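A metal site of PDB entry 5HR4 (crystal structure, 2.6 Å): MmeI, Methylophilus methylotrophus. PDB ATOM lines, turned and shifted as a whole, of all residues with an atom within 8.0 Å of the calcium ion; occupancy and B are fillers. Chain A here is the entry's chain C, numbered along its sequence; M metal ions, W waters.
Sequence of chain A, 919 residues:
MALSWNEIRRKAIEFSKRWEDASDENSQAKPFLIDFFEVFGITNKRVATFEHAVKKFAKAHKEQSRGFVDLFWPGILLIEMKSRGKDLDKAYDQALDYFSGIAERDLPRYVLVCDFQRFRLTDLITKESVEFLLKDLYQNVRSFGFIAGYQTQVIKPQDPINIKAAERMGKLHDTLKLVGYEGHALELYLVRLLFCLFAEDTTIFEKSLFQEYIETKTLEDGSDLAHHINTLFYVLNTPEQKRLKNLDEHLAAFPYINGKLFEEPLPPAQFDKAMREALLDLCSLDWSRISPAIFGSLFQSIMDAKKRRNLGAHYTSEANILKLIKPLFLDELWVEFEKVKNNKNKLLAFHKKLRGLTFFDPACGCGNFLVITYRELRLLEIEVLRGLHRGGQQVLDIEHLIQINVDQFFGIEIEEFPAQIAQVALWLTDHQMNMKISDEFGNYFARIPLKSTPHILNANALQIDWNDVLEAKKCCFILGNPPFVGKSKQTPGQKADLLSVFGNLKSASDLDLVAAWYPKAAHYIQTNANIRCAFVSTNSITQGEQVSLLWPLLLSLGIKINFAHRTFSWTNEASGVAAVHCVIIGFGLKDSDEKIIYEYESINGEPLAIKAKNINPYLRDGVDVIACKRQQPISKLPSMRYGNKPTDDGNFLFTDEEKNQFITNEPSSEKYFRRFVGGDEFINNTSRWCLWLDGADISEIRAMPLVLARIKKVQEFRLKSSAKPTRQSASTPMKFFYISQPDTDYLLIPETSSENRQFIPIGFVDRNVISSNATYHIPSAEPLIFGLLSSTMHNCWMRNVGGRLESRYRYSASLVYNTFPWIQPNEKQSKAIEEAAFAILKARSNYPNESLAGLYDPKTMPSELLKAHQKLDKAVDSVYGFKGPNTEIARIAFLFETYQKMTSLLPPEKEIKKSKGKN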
ATOM      1  N   GLN A 158     -19.113  11.608 -20.521  1.00  0.00           N
ATOM      2  CA  GLN A 158     -18.397  12.550 -19.673  1.00  0.00           C
ATOM      3  C   GLN A 158     -17.351  13.318 -20.473  1.00  0.00           C
ATOM      4  O   GLN A 158     -16.729  12.779 -21.388  1.00  0.00           O
ATOM      5  CB  GLN A 158     -17.735  11.808 -18.506  1.00  0.00           C
ATOM      6  CG  GLN A 158     -18.717  11.076 -17.595  1.00  0.00           C
ATOM      7  CD  GLN A 158     -18.070  10.513 -16.333  1.00  0.00           C
ATOM      8  OE1 GLN A 158     -16.933  10.060 -16.363  1.00  0.00           O
ATOM      9  NE2 GLN A 158     -18.797  10.563 -15.209  1.00  0.00           N
ATOM     10  N   ASP A 159     -17.154  14.588 -20.118  1.00  0.00           N
ATOM     11  CA  ASP A 159     -16.195  15.443 -20.830  1.00  0.00           C
ATOM     12  C   ASP A 159     -14.793  14.866 -20.703  1.00  0.00           C
ATOM     13  O   ASP A 159     -14.328  14.644 -19.580  1.00  0.00           O
ATOM     14  CB  ASP A 159     -16.212  16.872 -20.272  1.00  0.00           C
ATOM     15  CG  ASP A 159     -17.539  17.608 -20.503  1.00  0.00           C
ATOM     16  OD1 ASP A 159     -18.371  17.131 -21.305  1.00  0.00           O
ATOM     17  OD2 ASP A 159     -17.722  18.690 -19.894  1.00  0.00           O
ATOM     18  N   ILE A 161     -10.810  14.728 -20.315  1.00  0.00           N
ATOM     19  CA  ILE A 161      -9.947  15.643 -19.571  1.00  0.00           C
ATOM     20  C   ILE A 161      -9.101  16.460 -20.539  1.00  0.00           C
ATOM     21  O   ILE A 161      -8.768  16.010 -21.641  1.00  0.00           O
ATOM     22  CB  ILE A 161      -9.049  14.870 -18.589  1.00  0.00           C
ATOM     23  CG1 ILE A 161      -8.416  13.682 -19.292  1.00  0.00           C
ATOM     24  CG2 ILE A 161      -9.828  14.412 -17.381  1.00  0.00           C
ATOM     25  CD1 ILE A 161      -6.997  13.477 -18.893  1.00  0.00           C
ATOM     26  N   CYS A 196      -7.170   5.555  -9.638  1.00  0.00           N
ATOM     27  CA  CYS A 196      -8.602   5.327  -9.459  1.00  0.00           C
ATOM     28  C   CYS A 196      -9.419   6.134 -10.457  1.00  0.00           C
ATOM     29  O   CYS A 196     -10.409   5.628 -10.993  1.00  0.00           O
ATOM     30  CB  CYS A 196      -9.001   5.641  -8.017  1.00  0.00           C
ATOM     31  SG  CYS A 196      -8.387   4.418  -6.830  1.00  0.00           S
ATOM     32  N   LEU A 197      -9.013   7.377 -10.741  1.00  0.00           N
ATOM     33  CA  LEU A 197      -9.792   8.175 -11.701  1.00  0.00           C
ATOM     34  C   LEU A 197      -9.753   7.543 -13.081  1.00  0.00           C
ATOM     35  O   LEU A 197     -10.786   7.447 -13.753  1.00  0.00           O
ATOM     36  CB  LEU A 197      -9.281   9.614 -11.740  1.00  0.00           C
ATOM     37  CG  LEU A 197      -9.521  10.376 -10.433  1.00  0.00           C
ATOM     38  CD1 LEU A 197      -8.708  11.636 -10.429  1.00  0.00           C
ATOM     39  CD2 LEU A 197     -10.989  10.689 -10.273  1.00  0.00           C
ATOM     40  N   PHE A 198      -8.591   7.051 -13.493  1.00  0.00           N
ATOM     41  CA  PHE A 198      -8.491   6.348 -14.765  1.00  0.00           C
ATOM     42  C   PHE A 198      -9.282   5.040 -14.748  1.00  0.00           C
ATOM     43  O   PHE A 198      -9.889   4.653 -15.753  1.00  0.00           O
ATOM     44  CB  PHE A 198      -7.021   6.097 -15.087  1.00  0.00           C
ATOM     45  CG  PHE A 198      -6.791   5.225 -16.284  1.00  0.00           C
ATOM     46  CD1 PHE A 198      -6.837   5.760 -17.564  1.00  0.00           C
ATOM     47  CD2 PHE A 198      -6.546   3.853 -16.138  1.00  0.00           C
ATOM     48  CE1 PHE A 198      -6.613   4.957 -18.696  1.00  0.00           C
ATOM     49  CE2 PHE A 198      -6.324   3.050 -17.241  1.00  0.00           C
ATOM     50  CZ  PHE A 198      -6.362   3.604 -18.527  1.00  0.00           C
ATOM     51  N   ALA A 199      -9.286   4.349 -13.602  1.00  0.00           N
ATOM     52  CA  ALA A 199      -9.818   2.988 -13.555  1.00  0.00           C
ATOM     53  C   ALA A 199     -11.341   2.961 -13.683  1.00  0.00           C
ATOM     54  O   ALA A 199     -11.891   2.052 -14.314  1.00  0.00           O
ATOM     55  CB  ALA A 199      -9.388   2.279 -12.276  1.00  0.00           C
ATOM     56  N   GLU A 200     -12.043   3.930 -13.081  1.00  0.00           N
ATOM     57  CA  GLU A 200     -13.500   3.864 -13.156  1.00  0.00           C
ATOM     58  C   GLU A 200     -14.019   4.230 -14.534  1.00  0.00           C
ATOM     59  O   GLU A 200     -15.153   3.868 -14.878  1.00  0.00           O
ATOM     60  CB  GLU A 200     -14.142   4.751 -12.084  1.00  0.00           C
ATOM     61  CG  GLU A 200     -13.891   6.232 -12.239  1.00  0.00           C
ATOM     62  CD  GLU A 200     -14.551   7.015 -11.086  1.00  0.00           C
ATOM     63  OE1 GLU A 200     -15.458   6.419 -10.450  1.00  0.00           O
ATOM     64  OE2 GLU A 200     -14.178   8.198 -10.835  1.00  0.00           O
ATOM     65  N   ASP A 201     -13.206   4.915 -15.337  1.00  0.00           N
ATOM     66  CA  ASP A 201     -13.569   5.343 -16.683  1.00  0.00           C
ATOM     67  C   ASP A 201     -13.141   4.340 -17.749  1.00  0.00           C
ATOM     68  O   ASP A 201     -13.300   4.579 -18.945  1.00  0.00           O
ATOM     69  CB  ASP A 201     -12.945   6.708 -16.979  1.00  0.00           C
ATOM     70  CG  ASP A 201     -13.689   7.814 -16.306  1.00  0.00           C
ATOM     71  OD1 ASP A 201     -14.814   7.523 -15.847  1.00  0.00           O
ATOM     72  OD2 ASP A 201     -13.146   8.941 -16.237  1.00  0.00           O
ATOM     73  N   THR A 202     -12.576   3.238 -17.314  1.00  0.00           N
ATOM     74  CA  THR A 202     -12.234   2.115 -18.155  1.00  0.00           C
ATOM     75  C   THR A 202     -12.909   0.901 -17.526  1.00  0.00           C
ATOM     76  O   THR A 202     -13.783   1.034 -16.643  1.00  0.00           O
ATOM     77  CB  THR A 202     -10.709   2.014 -18.272  1.00  0.00           C
ATOM     78  OG1 THR A 202     -10.210   3.267 -18.784  1.00  0.00           O
ATOM     79  CG2 THR A 202     -10.319   0.914 -19.229  1.00  0.00           C
ATOM     80  N   LYS A 207     -17.872   0.815 -14.340  1.00  0.00           N
ATOM     81  CA  LYS A 207     -17.959   2.217 -14.737  1.00  0.00           C
ATOM     82  C   LYS A 207     -18.392   3.093 -13.575  1.00  0.00           C
ATOM     83  O   LYS A 207     -19.433   2.865 -12.953  1.00  0.00           O
ATOM     84  CB  LYS A 207     -18.933   2.369 -15.909  1.00  0.00           C
ATOM     85  CG  LYS A 207     -18.755   3.652 -16.696  1.00  0.00           C
ATOM     86  CD  LYS A 207     -19.017   3.466 -18.199  1.00  0.00           C
ATOM     87  CE  LYS A 207     -18.540   4.682 -19.011  1.00  0.00           C
ATOM     88  NZ  LYS A 207     -18.838   4.594 -20.478  1.00  0.00           N
ATOM     89  N   SER A 208     -17.556   4.072 -13.257  1.00  0.00           N
ATOM     90  CA  SER A 208     -17.844   5.110 -12.265  1.00  0.00           C
ATOM     91  C   SER A 208     -17.948   4.573 -10.839  1.00  0.00           C
ATOM     92  O   SER A 208     -18.529   5.227  -9.968  1.00  0.00           O
ATOM     93  CB  SER A 208     -19.120   5.869 -12.641  1.00  0.00           C
ATOM     94  OG  SER A 208     -18.899   6.682 -13.784  1.00  0.00           O
ATOM     95  N   GLN A 211     -16.507   6.986  -8.286  1.00  0.00           N
ATOM     96  CA  GLN A 211     -17.330   8.176  -8.105  1.00  0.00           C
ATOM     97  C   GLN A 211     -18.614   7.854  -7.366  1.00  0.00           C
ATOM     98  O   GLN A 211     -19.021   8.586  -6.454  1.00  0.00           O
ATOM     99  CB  GLN A 211     -17.657   8.835  -9.457  1.00  0.00           C
ATOM    100  CG  GLN A 211     -18.561  10.061  -9.295  1.00  0.00           C
ATOM    101  CD  GLN A 211     -18.911  10.721 -10.613  1.00  0.00           C
ATOM    102  OE1 GLN A 211     -18.140  10.668 -11.571  1.00  0.00           O
ATOM    103  NE2 GLN A 211     -20.087  11.351 -10.667  1.00  0.00           N
ATOM    104  N   LEU A 280     -14.672  14.916  -6.604  1.00  0.00           N
ATOM    105  CA  LEU A 280     -15.823  14.508  -7.403  1.00  0.00           C
ATOM    106  C   LEU A 280     -15.807  15.227  -8.753  1.00  0.00           C
ATOM    107  O   LEU A 280     -16.208  14.659  -9.778  1.00  0.00           O
ATOM    108  CB  LEU A 280     -17.111  14.805  -6.650  1.00  0.00           C
ATOM    109  CG  LEU A 280     -17.494  13.841  -5.543  1.00  0.00           C
ATOM    110  CD1 LEU A 280     -18.722  14.351  -4.788  1.00  0.00           C
ATOM    111  CD2 LEU A 280     -17.733  12.471  -6.136  1.00  0.00           C
ATOM    112  N   ASP A 281     -15.359  16.476  -8.758  1.00  0.00           N
ATOM    113  CA  ASP A 281     -15.155  17.216  -9.996  1.00  0.00           C
ATOM    114  C   ASP A 281     -14.248  16.447 -10.955  1.00  0.00           C
ATOM    115  O   ASP A 281     -14.562  16.305 -12.142  1.00  0.00           O
ATOM    116  CB  ASP A 281     -14.568  18.572  -9.664  1.00  0.00           C
ATOM    117  CG  ASP A 281     -15.057  19.618 -10.564  1.00  0.00           C
ATOM    118  OD1 ASP A 281     -14.503  19.721 -11.681  1.00  0.00           O
ATOM    119  OD2 ASP A 281     -15.982  20.353 -10.138  1.00  0.00           O
ATOM    120  N   LEU A 282     -13.106  15.971 -10.454  1.00  0.00           N
ATOM    121  CA  LEU A 282     -12.206  15.200 -11.300  1.00  0.00           C
ATOM    122  C   LEU A 282     -12.879  13.903 -11.764  1.00  0.00           C
ATOM    123  O   LEU A 282     -12.686  13.477 -12.910  1.00  0.00           O
ATOM    124  CB  LEU A 282     -10.905  14.920 -10.556  1.00  0.00           C
ATOM    125  CG  LEU A 282      -9.975  16.125 -10.326  1.00  0.00           C
ATOM    126  CD1 LEU A 282      -8.748  15.705  -9.534  1.00  0.00           C
ATOM    127  CD2 LEU A 282      -9.543  16.724 -11.652  1.00  0.00           C
ATOM    128  N   CYS A 283     -13.680  13.280 -10.895  1.00  0.00           N
ATOM    129  CA  CYS A 283     -14.329  12.022 -11.279  1.00  0.00           C
ATOM    130  C   CYS A 283     -15.239  12.217 -12.467  1.00  0.00           C
ATOM    131  O   CYS A 283     -15.332  11.346 -13.344  1.00  0.00           O
ATOM    132  CB  CYS A 283     -15.128  11.437 -10.118  1.00  0.00           C
ATOM    133  SG  CYS A 283     -14.161  10.846  -8.744  1.00  0.00           S
ATOM    134  N   SER A 284     -15.954  13.349 -12.529  1.00  0.00           N
ATOM    135  CA  SER A 284     -16.961  13.492 -13.561  1.00  0.00           C
ATOM    136  C   SER A 284     -16.369  13.624 -14.959  1.00  0.00           C
ATOM    137  O   SER A 284     -17.108  13.486 -15.931  1.00  0.00           O
ATOM    138  CB  SER A 284     -17.864  14.688 -13.265  1.00  0.00           C
ATOM    139  OG  SER A 284     -17.145  15.894 -13.374  1.00  0.00           O
ATOM    140  N   LEU A 285     -15.058  13.856 -15.088  1.00  0.00           N
ATOM    141  CA  LEU A 285     -14.408  13.858 -16.393  1.00  0.00           C
ATOM    142  C   LEU A 285     -14.073  12.422 -16.816  1.00  0.00           C
ATOM    143  O   LEU A 285     -14.124  11.477 -16.034  1.00  0.00           O
ATOM    144  CB  LEU A 285     -13.159  14.718 -16.363  1.00  0.00           C
ATOM    145  CG  LEU A 285     -13.364  16.139 -15.846  1.00  0.00           C
ATOM    146  CD1 LEU A 285     -12.046  16.908 -15.813  1.00  0.00           C
ATOM    147  CD2 LEU A 285     -14.382  16.879 -16.681  1.00  0.00           C
ATOM    148  N   ASP A 286     -13.707  12.275 -18.093  1.00  0.00           N
ATOM    149  CA  ASP A 286     -13.323  10.987 -18.645  1.00  0.00           C
ATOM    150  C   ASP A 286     -11.796  10.945 -18.718  1.00  0.00           C
ATOM    151  O   ASP A 286     -11.184  11.699 -19.489  1.00  0.00           O
ATOM    152  CB  ASP A 286     -13.961  10.780 -20.024  1.00  0.00           C
ATOM    153  CG  ASP A 286     -13.765   9.364 -20.555  1.00  0.00           C
ATOM    154  OD1 ASP A 286     -13.500   8.443 -19.759  1.00  0.00           O
ATOM    155  OD2 ASP A 286     -13.902   9.171 -21.795  1.00  0.00           O
ATOM    156  N   TRP A 287     -11.184  10.097 -17.904  1.00  0.00           N
ATOM    157  CA  TRP A 287      -9.737   9.960 -17.871  1.00  0.00           C
ATOM    158  C   TRP A 287      -9.228   8.974 -18.896  1.00  0.00           C
ATOM    159  O   TRP A 287      -8.017   8.713 -18.952  1.00  0.00           O
ATOM    160  CB  TRP A 287      -9.284   9.574 -16.455  1.00  0.00           C
ATOM    161  CG  TRP A 287      -9.556  10.711 -15.566  1.00  0.00           C
ATOM    162  CD1 TRP A 287     -10.770  11.091 -15.097  1.00  0.00           C
ATOM    163  CD2 TRP A 287      -8.629  11.708 -15.157  1.00  0.00           C
ATOM    164  NE1 TRP A 287     -10.654  12.246 -14.374  1.00  0.00           N
ATOM    165  CE2 TRP A 287      -9.353  12.646 -14.387  1.00  0.00           C
ATOM    166  CE3 TRP A 287      -7.259  11.894 -15.333  1.00  0.00           C
ATOM    167  CZ2 TRP A 287      -8.741  13.746 -13.776  1.00  0.00           C
ATOM    168  CZ3 TRP A 287      -6.659  12.991 -14.730  1.00  0.00           C
ATOM    169  CH2 TRP A 287      -7.406  13.901 -13.969  1.00  0.00           C
ATOM    170  N   SER A 288     -10.125   8.466 -19.746  1.00  0.00           N
ATOM    171  CA  SER A 288      -9.807   7.338 -20.603  1.00  0.00           C
ATOM    172  C   SER A 288      -8.645   7.631 -21.534  1.00  0.00           C
ATOM    173  O   SER A 288      -7.759   6.785 -21.731  1.00  0.00           O
ATOM    174  CB  SER A 288     -11.046   6.954 -21.408  1.00  0.00           C
ATOM    175  OG  SER A 288     -10.875   5.638 -21.882  1.00  0.00           O
HETATM  176 CA    CA M   1     -15.044   9.759 -14.937  1.00  0.00          CA
HETATM  177  O   HOH W   1     -16.524   8.663 -13.393  1.00  0.00           O
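The side-chain carboxylate (OD2) of Asp 201 lies close to the backbone NH (N) of Trp 287 (2.8 Å). NE2 of Gln 158 lies close to O of Ser 284, 3.5 Å away. The side-chain sulfur (SG) of Cys 283 is in hydrogen-bond range of the side-chain carboxylate (OE2) of Glu 200, 3.4 Å away. The side-chain amide oxygen (OE1) of Gln 211 sits close to the backbone carbonyl oxygen (O) of Cys 283 (3.4 Å).
Four residues have an atom within 4 Å of the calcium ion: Gln 158, Asp 201, Cys 283 and Leu 285.
The backbone carbonyl oxygen (O) of Leu 285 is bound to the calcium ion (2.2 Å). O of Cys 283 binds the calcium ion, 2.3 Å away. The side-chain amide oxygen (OE1) of Gln 158 binds the calcium ion (2.4 Å). The calcium ion is bound by water W1. OD1 of Asp 201 is bound to the calcium ion (2.4 Å). The calcium ion is bound by OD2 of Asp 201 (2.4 Å). The calcium ion has six donor atoms within binding distance.
Water W1 lies within hydrogen-bond range of the side-chain hydroxyl of Ser 208 (3.1 Å), the side-chain amide oxygen of Gln 211 (3.2 Å) and the side-chain amide nitrogen of Gln 158 (3.5 Å).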
